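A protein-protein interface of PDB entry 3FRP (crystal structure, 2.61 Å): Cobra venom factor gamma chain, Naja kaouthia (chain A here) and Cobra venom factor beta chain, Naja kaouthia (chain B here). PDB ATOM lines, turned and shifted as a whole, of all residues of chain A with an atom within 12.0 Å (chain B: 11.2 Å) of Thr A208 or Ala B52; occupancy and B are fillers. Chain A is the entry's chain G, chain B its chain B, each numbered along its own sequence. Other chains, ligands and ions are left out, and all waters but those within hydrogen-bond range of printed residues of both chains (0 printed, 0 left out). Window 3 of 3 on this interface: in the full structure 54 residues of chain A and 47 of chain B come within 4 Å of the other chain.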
ATOM      1  N   LYS A 197      -8.271  11.536  15.828  1.00  0.00           N
ATOM      2  CA  LYS A 197      -7.553  12.828  15.676  1.00  0.00           C
ATOM      3  C   LYS A 197      -8.406  14.052  16.048  1.00  0.00           C
ATOM      4  O   LYS A 197      -9.628  13.947  16.185  1.00  0.00           O
ATOM      5  CB  LYS A 197      -7.033  13.016  14.248  1.00  0.00           C
ATOM      6  CG  LYS A 197      -6.024  11.983  13.771  1.00  0.00           C
ATOM      7  CD  LYS A 197      -5.562  12.263  12.334  1.00  0.00           C
ATOM      8  CE  LYS A 197      -6.697  12.750  11.425  1.00  0.00           C
ATOM      9  NZ  LYS A 197      -7.782  11.748  11.238  1.00  0.00           N
ATOM     10  N   LEU A 198      -7.750  15.208  16.180  1.00  0.00           N
ATOM     11  CA  LEU A 198      -8.405  16.465  16.569  1.00  0.00           C
ATOM     12  C   LEU A 198      -8.069  17.608  15.591  1.00  0.00           C
ATOM     13  O   LEU A 198      -7.203  17.440  14.731  1.00  0.00           O
ATOM     14  CB  LEU A 198      -8.004  16.824  18.003  1.00  0.00           C
ATOM     15  CG  LEU A 198      -8.496  15.879  19.109  1.00  0.00           C
ATOM     16  CD1 LEU A 198      -7.359  15.444  20.040  1.00  0.00           C
ATOM     17  CD2 LEU A 198      -9.655  16.501  19.887  1.00  0.00           C
ATOM     18  N   ASP A 199      -8.739  18.762  15.729  1.00  0.00           N
ATOM     19  CA  ASP A 199      -8.599  19.902  14.778  1.00  0.00           C
ATOM     20  C   ASP A 199      -8.064  21.254  15.350  1.00  0.00           C
ATOM     21  O   ASP A 199      -8.848  22.200  15.477  1.00  0.00           O
ATOM     22  CB  ASP A 199      -9.956  20.186  14.092  1.00  0.00           C
ATOM     23  CG  ASP A 199     -10.304  19.192  12.985  1.00  0.00           C
ATOM     24  OD1 ASP A 199      -9.453  18.348  12.611  1.00  0.00           O
ATOM     25  OD2 ASP A 199     -11.449  19.274  12.478  1.00  0.00           O
ATOM     26  N   PRO A 200      -6.741  21.373  15.654  1.00  0.00           N
ATOM     27  CA  PRO A 200      -6.250  22.649  16.207  1.00  0.00           C
ATOM     28  C   PRO A 200      -5.855  23.667  15.132  1.00  0.00           C
ATOM     29  O   PRO A 200      -6.724  24.193  14.434  1.00  0.00           O
ATOM     30  CB  PRO A 200      -5.008  22.222  16.989  1.00  0.00           C
ATOM     31  CG  PRO A 200      -4.456  21.079  16.197  1.00  0.00           C
ATOM     32  CD  PRO A 200      -5.646  20.385  15.542  1.00  0.00           C
ATOM     33  N   THR A 208      -5.344  26.993   7.432  1.00  0.00           N
ATOM     34  CA  THR A 208      -5.854  25.712   6.959  1.00  0.00           C
ATOM     35  C   THR A 208      -4.978  24.515   7.350  1.00  0.00           C
ATOM     36  O   THR A 208      -3.819  24.409   6.948  1.00  0.00           O
ATOM     37  CB  THR A 208      -6.086  25.745   5.444  1.00  0.00           C
ATOM     38  N   GLN A 209      -5.564  23.623   8.143  1.00  0.00           N
ATOM     39  CA  GLN A 209      -4.920  22.397   8.600  1.00  0.00           C
ATOM     40  C   GLN A 209      -5.463  21.204   7.823  1.00  0.00           C
ATOM     41  O   GLN A 209      -6.646  21.155   7.515  1.00  0.00           O
ATOM     42  CB  GLN A 209      -5.200  22.214  10.087  1.00  0.00           C
ATOM     43  CG  GLN A 209      -4.815  20.861  10.631  1.00  0.00           C
ATOM     44  CD  GLN A 209      -5.709  20.421  11.773  1.00  0.00           C
ATOM     45  OE1 GLN A 209      -6.423  21.228  12.386  1.00  0.00           O
ATOM     46  NE2 GLN A 209      -5.674  19.131  12.071  1.00  0.00           N
ATOM     47  N   LEU A 210      -4.604  20.241   7.515  1.00  0.00           N
ATOM     48  CA  LEU A 210      -5.023  19.073   6.742  1.00  0.00           C
ATOM     49  C   LEU A 210      -4.450  17.790   7.322  1.00  0.00           C
ATOM     50  O   LEU A 210      -3.505  17.852   8.109  1.00  0.00           O
ATOM     51  CB  LEU A 210      -4.625  19.233   5.267  1.00  0.00           C
ATOM     52  CG  LEU A 210      -3.155  19.115   4.864  1.00  0.00           C
ATOM     53  CD1 LEU A 210      -2.898  17.762   4.195  1.00  0.00           C
ATOM     54  CD2 LEU A 210      -2.735  20.263   3.939  1.00  0.00           C
ATOM     55  N   GLU A 211      -5.022  16.644   6.937  1.00  0.00           N
ATOM     56  CA  GLU A 211      -4.495  15.327   7.348  1.00  0.00           C
ATOM     57  C   GLU A 211      -4.852  14.092   6.486  1.00  0.00           C
ATOM     58  O   GLU A 211      -6.019  13.849   6.167  1.00  0.00           O
ATOM     59  CB  GLU A 211      -4.789  15.061   8.828  1.00  0.00           C
ATOM     60  CG  GLU A 211      -3.535  15.145   9.680  1.00  0.00           C
ATOM     61  CD  GLU A 211      -3.820  15.464  11.121  1.00  0.00           C
ATOM     62  OE1 GLU A 211      -4.662  16.356  11.383  1.00  0.00           O
ATOM     63  OE2 GLU A 211      -3.185  14.824  11.993  1.00  0.00           O
ATOM     64  N   VAL A 212      -3.827  13.316   6.128  1.00  0.00           N
ATOM     65  CA  VAL A 212      -4.007  12.069   5.376  1.00  0.00           C
ATOM     66  C   VAL A 212      -4.026  10.862   6.333  1.00  0.00           C
ATOM     67  O   VAL A 212      -3.220  10.775   7.268  1.00  0.00           O
ATOM     68  CB  VAL A 212      -2.942  11.899   4.222  1.00  0.00           C
ATOM     69  CG1 VAL A 212      -3.035  10.516   3.546  1.00  0.00           C
ATOM     70  CG2 VAL A 212      -3.096  12.997   3.163  1.00  0.00           C
ATOM     71  N   ILE A 213      -4.975   9.955   6.097  1.00  0.00           N
ATOM     72  CA  ILE A 213      -5.155   8.728   6.884  1.00  0.00           C
ATOM     73  C   ILE A 213      -5.129   7.541   5.906  1.00  0.00           C
ATOM     74  O   ILE A 213      -6.115   7.280   5.211  1.00  0.00           O
ATOM     75  CB  ILE A 213      -6.501   8.749   7.676  1.00  0.00           C
ATOM     76  CG1 ILE A 213      -6.718  10.106   8.365  1.00  0.00           C
ATOM     77  CG2 ILE A 213      -6.556   7.603   8.682  1.00  0.00           C
ATOM     78  CD1 ILE A 213      -8.114  10.673   8.183  1.00  0.00           C
ATOM     79  N   ILE A 233     -16.956  13.148  12.382  1.00  0.00           N
ATOM     80  CA  ILE A 233     -16.311  14.386  12.822  1.00  0.00           C
ATOM     81  C   ILE A 233     -17.268  15.165  13.728  1.00  0.00           C
ATOM     82  O   ILE A 233     -18.462  15.275  13.428  1.00  0.00           O
ATOM     83  CB  ILE A 233     -15.869  15.221  11.626  1.00  0.00           C
ATOM     84  N   GLN A 234     -16.733  15.694  14.829  1.00  0.00           N
ATOM     85  CA  GLN A 234     -17.528  16.334  15.893  1.00  0.00           C
ATOM     86  C   GLN A 234     -17.082  17.771  16.185  1.00  0.00           C
ATOM     87  O   GLN A 234     -16.136  18.263  15.572  1.00  0.00           O
ATOM     88  CB  GLN A 234     -17.464  15.506  17.184  1.00  0.00           C
ATOM     89  CG  GLN A 234     -18.221  14.167  17.145  1.00  0.00           C
ATOM     90  CD  GLN A 234     -17.983  13.305  18.396  1.00  0.00           C
ATOM     91  OE1 GLN A 234     -16.839  13.082  18.811  1.00  0.00           O
ATOM     92  NE2 GLN A 234     -19.070  12.814  18.993  1.00  0.00           N
ATOM     93  N   GLY A 235     -17.753  18.429  17.134  1.00  0.00           N
ATOM     94  CA  GLY A 235     -17.577  19.868  17.375  1.00  0.00           C
ATOM     95  C   GLY A 235     -16.564  20.261  18.437  1.00  0.00           C
ATOM     96  O   GLY A 235     -15.604  20.988  18.153  1.00  0.00           O
ATOM     97  N   LEU B  10     -16.627  28.230  18.134  1.00  0.00           N
ATOM     98  CA  LEU B  10     -16.169  27.525  16.900  1.00  0.00           C
ATOM     99  C   LEU B  10     -16.737  28.204  15.657  1.00  0.00           C
ATOM    100  O   LEU B  10     -17.938  28.491  15.590  1.00  0.00           O
ATOM    101  CB  LEU B  10     -16.576  26.044  16.919  1.00  0.00           C
ATOM    102  CG  LEU B  10     -16.209  25.160  18.112  1.00  0.00           C
ATOM    103  CD1 LEU B  10     -17.003  23.876  18.005  1.00  0.00           C
ATOM    104  CD2 LEU B  10     -14.704  24.878  18.212  1.00  0.00           C
ATOM    105  N   ASN B  11     -15.862  28.452  14.683  1.00  0.00           N
ATOM    106  CA  ASN B  11     -16.224  29.120  13.434  1.00  0.00           C
ATOM    107  C   ASN B  11     -15.539  28.427  12.244  1.00  0.00           C
ATOM    108  O   ASN B  11     -14.802  29.051  11.461  1.00  0.00           O
ATOM    109  CB  ASN B  11     -15.858  30.608  13.521  1.00  0.00           C
ATOM    110  CG  ASN B  11     -16.283  31.390  12.296  1.00  0.00           C
ATOM    111  OD1 ASN B  11     -17.293  31.081  11.657  1.00  0.00           O
ATOM    112  ND2 ASN B  11     -15.503  32.411  11.957  1.00  0.00           N
ATOM    113  N   LEU B  12     -15.794  27.126  12.119  1.00  0.00           N
ATOM    114  CA  LEU B  12     -15.072  26.275  11.176  1.00  0.00           C
ATOM    115  C   LEU B  12     -15.678  26.233   9.763  1.00  0.00           C
ATOM    116  O   LEU B  12     -16.763  26.785   9.504  1.00  0.00           O
ATOM    117  CB  LEU B  12     -14.902  24.857  11.752  1.00  0.00           C
ATOM    118  CG  LEU B  12     -14.089  24.692  13.052  1.00  0.00           C
ATOM    119  CD1 LEU B  12     -14.356  23.344  13.726  1.00  0.00           C
ATOM    120  CD2 LEU B  12     -12.572  24.911  12.845  1.00  0.00           C
ATOM    121  N   ASP B  13     -14.934  25.593   8.860  1.00  0.00           N
ATOM    122  CA  ASP B  13     -15.325  25.362   7.471  1.00  0.00           C
ATOM    123  C   ASP B  13     -14.498  24.172   6.975  1.00  0.00           C
ATOM    124  O   ASP B  13     -13.299  24.298   6.733  1.00  0.00           O
ATOM    125  CB  ASP B  13     -15.081  26.622   6.631  1.00  0.00           C
ATOM    126  CG  ASP B  13     -15.253  26.389   5.139  1.00  0.00           C
ATOM    127  OD1 ASP B  13     -15.576  25.262   4.723  1.00  0.00           O
ATOM    128  OD2 ASP B  13     -15.061  27.351   4.369  1.00  0.00           O
ATOM    129  N   ILE B  14     -15.144  23.015   6.843  1.00  0.00           N
ATOM    130  CA  ILE B  14     -14.440  21.762   6.553  1.00  0.00           C
ATOM    131  C   ILE B  14     -14.636  21.283   5.112  1.00  0.00           C
ATOM    132  O   ILE B  14     -15.521  21.759   4.399  1.00  0.00           O
ATOM    133  CB  ILE B  14     -14.820  20.624   7.565  1.00  0.00           C
ATOM    134  CG1 ILE B  14     -14.656  21.083   9.024  1.00  0.00           C
ATOM    135  CG2 ILE B  14     -14.017  19.335   7.310  1.00  0.00           C
ATOM    136  CD1 ILE B  14     -13.227  21.445   9.449  1.00  0.00           C
ATOM    137  N   THR B  15     -13.774  20.349   4.703  1.00  0.00           N
ATOM    138  CA  THR B  15     -13.795  19.734   3.379  1.00  0.00           C
ATOM    139  C   THR B  15     -13.014  18.403   3.357  1.00  0.00           C
ATOM    140  O   THR B  15     -11.819  18.372   3.640  1.00  0.00           O
ATOM    141  CB  THR B  15     -13.297  20.711   2.268  1.00  0.00           C
ATOM    142  OG1 THR B  15     -12.719  19.958   1.196  1.00  0.00           O
ATOM    143  CG2 THR B  15     -12.258  21.725   2.804  1.00  0.00           C
ATOM    144  N   ILE B  16     -13.703  17.309   3.021  1.00  0.00           N
ATOM    145  CA  ILE B  16     -13.097  15.962   3.008  1.00  0.00           C
ATOM    146  C   ILE B  16     -12.947  15.368   1.598  1.00  0.00           C
ATOM    147  O   ILE B  16     -13.873  15.418   0.787  1.00  0.00           O
ATOM    148  CB  ILE B  16     -13.865  14.951   3.915  1.00  0.00           C
ATOM    149  CG1 ILE B  16     -14.214  15.574   5.276  1.00  0.00           C
ATOM    150  CG2 ILE B  16     -13.054  13.663   4.094  1.00  0.00           C
ATOM    151  CD1 ILE B  16     -15.111  14.726   6.151  1.00  0.00           C
ATOM    152  N   GLU B  17     -11.772  14.800   1.333  1.00  0.00           N
ATOM    153  CA  GLU B  17     -11.452  14.199   0.046  1.00  0.00           C
ATOM    154  C   GLU B  17     -11.450  12.674   0.107  1.00  0.00           C
ATOM    155  O   GLU B  17     -10.801  12.069   0.959  1.00  0.00           O
ATOM    156  CB  GLU B  17     -10.092  14.692  -0.455  1.00  0.00           C
ATOM    157  CG  GLU B  17     -10.097  16.079  -1.103  1.00  0.00           C
ATOM    158  CD  GLU B  17      -8.735  16.452  -1.699  1.00  0.00           C
ATOM    159  OE1 GLU B  17      -7.718  16.400  -0.969  1.00  0.00           O
ATOM    160  OE2 GLU B  17      -8.681  16.805  -2.899  1.00  0.00           O
ATOM    161  N   ILE B  25     -16.439  16.449  -0.206  1.00  0.00           N
ATOM    162  CA  ILE B  25     -17.601  16.917   0.569  1.00  0.00           C
ATOM    163  C   ILE B  25     -17.234  17.981   1.619  1.00  0.00           C
ATOM    164  O   ILE B  25     -16.193  17.874   2.262  1.00  0.00           O
ATOM    165  CB  ILE B  25     -18.307  15.732   1.224  1.00  0.00           C
ATOM    166  N   ARG B  26     -18.101  18.989   1.783  1.00  0.00           N
ATOM    167  CA  ARG B  26     -17.875  20.127   2.696  1.00  0.00           C
ATOM    168  C   ARG B  26     -19.031  20.350   3.683  1.00  0.00           C
ATOM    169  O   ARG B  26     -20.194  20.198   3.322  1.00  0.00           O
ATOM    170  CB  ARG B  26     -17.602  21.408   1.896  1.00  0.00           C
ATOM    171  N   TYR B  27     -18.704  20.722   4.920  1.00  0.00           N
ATOM    172  CA  TYR B  27     -19.708  20.958   5.967  1.00  0.00           C
ATOM    173  C   TYR B  27     -19.253  22.004   7.005  1.00  0.00           C
ATOM    174  O   TYR B  27     -18.191  21.858   7.619  1.00  0.00           O
ATOM    175  CB  TYR B  27     -20.088  19.639   6.646  1.00  0.00           C
ATOM    176  N   ARG B  28     -20.074  23.045   7.194  1.00  0.00           N
ATOM    177  CA  ARG B  28     -19.759  24.204   8.064  1.00  0.00           C
ATOM    178  C   ARG B  28     -19.997  23.946   9.557  1.00  0.00           C
ATOM    179  O   ARG B  28     -21.095  24.197  10.063  1.00  0.00           O
ATOM    180  CB  ARG B  28     -20.590  25.435   7.656  1.00  0.00           C
ATOM    181  CG  ARG B  28     -20.254  26.045   6.314  1.00  0.00           C
ATOM    182  CD  ARG B  28     -20.658  27.511   6.282  1.00  0.00           C
ATOM    183  NE  ARG B  28     -19.677  28.323   5.559  1.00  0.00           N
ATOM    184  CZ  ARG B  28     -18.552  28.817   6.085  1.00  0.00           C
ATOM    185  NH1 ARG B  28     -17.738  29.541   5.327  1.00  0.00           N
ATOM    186  NH2 ARG B  28     -18.228  28.594   7.360  1.00  0.00           N
ATOM    187  N   ILE B  29     -18.974  23.471  10.261  1.00  0.00           N
ATOM    188  CA  ILE B  29     -19.070  23.248  11.709  1.00  0.00           C
ATOM    189  C   ILE B  29     -19.045  24.568  12.502  1.00  0.00           C
ATOM    190  O   ILE B  29     -17.980  25.158  12.725  1.00  0.00           O
ATOM    191  CB  ILE B  29     -17.967  22.300  12.179  1.00  0.00           C
ATOM    192  N   ILE B  48      -7.954   8.735   3.473  1.00  0.00           N
ATOM    193  CA  ILE B  48      -8.786   9.944   3.511  1.00  0.00           C
ATOM    194  C   ILE B  48      -7.898  11.196   3.506  1.00  0.00           C
ATOM    195  O   ILE B  48      -6.791  11.172   4.045  1.00  0.00           O
ATOM    196  CB  ILE B  48      -9.673   9.936   4.761  1.00  0.00           C
ATOM    197  N   THR B  49      -8.373  12.281   2.897  1.00  0.00           N
ATOM    198  CA  THR B  49      -7.697  13.582   3.036  1.00  0.00           C
ATOM    199  C   THR B  49      -8.668  14.633   3.593  1.00  0.00           C
ATOM    200  O   THR B  49      -9.669  14.966   2.957  1.00  0.00           O
ATOM    201  CB  THR B  49      -7.019  14.077   1.719  1.00  0.00           C
ATOM    202  OG1 THR B  49      -6.332  12.994   1.084  1.00  0.00           O
ATOM    203  CG2 THR B  49      -6.009  15.172   2.011  1.00  0.00           C
ATOM    204  N   VAL B  50      -8.353  15.127   4.794  1.00  0.00           N
ATOM    205  CA  VAL B  50      -9.171  16.107   5.530  1.00  0.00           C
ATOM    206  C   VAL B  50      -8.565  17.511   5.385  1.00  0.00           C
ATOM    207  O   VAL B  50      -7.334  17.647   5.317  1.00  0.00           O
ATOM    208  CB  VAL B  50      -9.232  15.764   7.050  1.00  0.00           C
ATOM    209  CG1 VAL B  50     -10.453  16.397   7.717  1.00  0.00           C
ATOM    210  CG2 VAL B  50      -9.227  14.268   7.260  1.00  0.00           C
ATOM    211  N   THR B  51      -9.420  18.538   5.337  1.00  0.00           N
ATOM    212  CA  THR B  51      -8.972  19.944   5.327  1.00  0.00           C
ATOM    213  C   THR B  51      -9.853  20.799   6.252  1.00  0.00           C
ATOM    214  O   THR B  51     -11.087  20.763   6.159  1.00  0.00           O
ATOM    215  CB  THR B  51      -8.875  20.544   3.877  1.00  0.00           C
ATOM    216  OG1 THR B  51      -7.768  19.954   3.185  1.00  0.00           O
ATOM    217  CG2 THR B  51      -8.651  22.054   3.905  1.00  0.00           C
ATOM    218  N   ALA B  52      -9.199  21.538   7.153  1.00  0.00           N
ATOM    219  CA  ALA B  52      -9.861  22.449   8.090  1.00  0.00           C
ATOM    220  C   ALA B  52      -9.546  23.899   7.731  1.00  0.00           C
ATOM    221  O   ALA B  52      -8.699  24.162   6.882  1.00  0.00           O
ATOM    222  CB  ALA B  52      -9.436  22.143   9.518  1.00  0.00           C
ATOM    223  N   SER B  53     -10.230  24.842   8.371  1.00  0.00           N
ATOM    224  CA  SER B  53     -10.144  26.238   7.965  1.00  0.00           C
ATOM    225  C   SER B  53     -10.972  27.118   8.896  1.00  0.00           C
ATOM    226  O   SER B  53     -11.449  26.616   9.937  1.00  0.00           O
ATOM    227  CB  SER B  53     -10.627  26.385   6.514  1.00  0.00           C
ATOM    228  OG  SER B  53     -10.569  27.725   6.079  1.00  0.00           O
ATOM    229  N   ALA B  58     -12.881  20.525  17.249  1.00  0.00           N
ATOM    230  CA  ALA B  58     -13.414  19.394  16.487  1.00  0.00           C
ATOM    231  C   ALA B  58     -12.516  18.147  16.503  1.00  0.00           C
ATOM    232  O   ALA B  58     -11.289  18.250  16.462  1.00  0.00           O
ATOM    233  CB  ALA B  58     -13.719  19.812  15.063  1.00  0.00           C
ATOM    234  N   THR B  59     -13.148  16.974  16.558  1.00  0.00           N
ATOM    235  CA  THR B  59     -12.453  15.676  16.585  1.00  0.00           C
ATOM    236  C   THR B  59     -13.045  14.692  15.577  1.00  0.00           C
ATOM    237  O   THR B  59     -14.258  14.677  15.343  1.00  0.00           O
ATOM    238  CB  THR B  59     -12.449  15.017  18.013  1.00  0.00           C
ATOM    239  OG1 THR B  59     -12.186  13.604  17.909  1.00  0.00           O
ATOM    240  CG2 THR B  59     -13.781  15.223  18.729  1.00  0.00           C
ATOM    241  N   MET B  60     -12.184  13.857  14.998  1.00  0.00           N
ATOM    242  CA  MET B  60     -12.610  12.885  13.994  1.00  0.00           C
ATOM    243  C   MET B  60     -12.291  11.445  14.396  1.00  0.00           C
ATOM    244  O   MET B  60     -11.195  11.168  14.883  1.00  0.00           O
ATOM    245  CB  MET B  60     -11.976  13.213  12.646  1.00  0.00           C
ATOM    246  CG  MET B  60     -12.019  12.075  11.648  1.00  0.00           C
ATOM    247  SD  MET B  60     -11.451  12.560  10.019  1.00  0.00           S
ATOM    248  CE  MET B  60     -12.792  13.660   9.533  1.00  0.00           C
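Of the 13 printed residues of chain A, 12 touch a printed residue of chain B.
Printed residues of chain A that touch a printed residue of chain B: Lys A197, Leu A198, Asp A199, Thr A208, Gln A209, Leu A210, Glu A211, Val A212, Ile A213, Ile A233, Gln A234 and Gly A235.
Hydrophobic or aromatic side chains of chain A within 4 Å of the printed part of chain B: Leu A198, Leu A210, Val A212 and Ile A213.
Of the 22 printed residues of chain B, 9 touch a printed residue of chain A.
Printed residues of chain B that touch a printed residue of chain A: Leu B10, Ile B48, Thr B49, Val B50, Thr B51, Ala B52, Ala B58, Thr B59 and Met B60.
The side-chain amide nitrogen of Gln A209 is in hydrogen-bond range of the side-chain carboxylate of Glu A211, at 3.0 Å.
O of Thr B15 is in hydrogen-bond range of N of Thr B51 (2.9 Å).
The backbone carbonyl oxygen (O) of Thr B49 is in hydrogen-bond range of the backbone NH (N) of Glu B17 (2.7 Å).
The side-chain hydroxyl (OG1) of Thr B59 is in hydrogen-bond range of the backbone carbonyl oxygen (O) of Lys A197, at 3.1 Å.
The backbone carbonyl oxygen of Lys A197 lies within hydrogen-bond range of the backbone NH of Met B60.
O of Ala B58 lies within hydrogen-bond range of N of Asp A199, at 2.7 Å.
The backbone carbonyl oxygen of Gln A209 is in hydrogen-bond range of the backbone NH of Ala B52 (2.6 Å).
The backbone carbonyl oxygen (O) of Glu A211 is in hydrogen-bond range of the backbone NH (N) of Val B50, 3.0 Å away.
The backbone carbonyl oxygen of Ile A213 lies within hydrogen-bond range of the backbone NH of Ile B48 (2.9 Å).
N of Gln A234 is in hydrogen-bond range of O of Thr B59.
The backbone carbonyl oxygen (O) of Gly A235 is in hydrogen-bond range of the backbone NH (N) of Ala B58 (2.9 Å).
Printed residues of chain B within 4 Å of Lys A197: Thr B59 (3.1 Å) and Met B60 (2.8 Å).
Of chain B, only Ala B58 (2.7 Å) comes within 4 Å of Asp A199.
Thr A208 touches just one residue of chain B: Ala B52.
Gln A209 touches just these residues of chain B: Thr B51 and Ala B52.
Of the printed residues of chain B, Glu A211 touches Ile B48, Thr B49 and Val B50.
Of the printed residues of chain B, Val A212 touches Ile B48 and Thr B49.
Of the printed residues of chain B, Gly A235 touches Leu B10 and Ala B58.
No residue of chain A comes within 4 Å of Asp B13.
No residue of chain A comes within 4 Å of Ile B14.
Thr B51 touches just these residues of chain A: Gln A209 and Leu A210.
Of the printed residues of chain A, Ala B52 touches Thr A208 (3.2 Å) and Gln A209 (2.6 Å).
No residue of chain A comes within 4 Å of Ser B53.
The nearest residue of chain A that does not touch Ala B52 is Asp A199 (4.6 Å).
The nearest printed residue of chain A that does not touch Met B60 is Ile A233 (4.04 Å).
Among the printed residues, merely in contact across the chains: Gln A234 with Ala B58, Leu A210 with Val B50, Gly A235 with Leu B10, Val A212 with Ile B48, Thr A208 with Ala B52, Ile A233 with Thr B59, Leu A198 with Ala B58, Gln A209 with Thr B51, Glu A211 with Ile B48, Glu A211 with Thr B49, Leu A198 with Thr B59, Val A212 with Thr B49, Leu A210 with Thr B51 and Ile A213 with Val B50.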
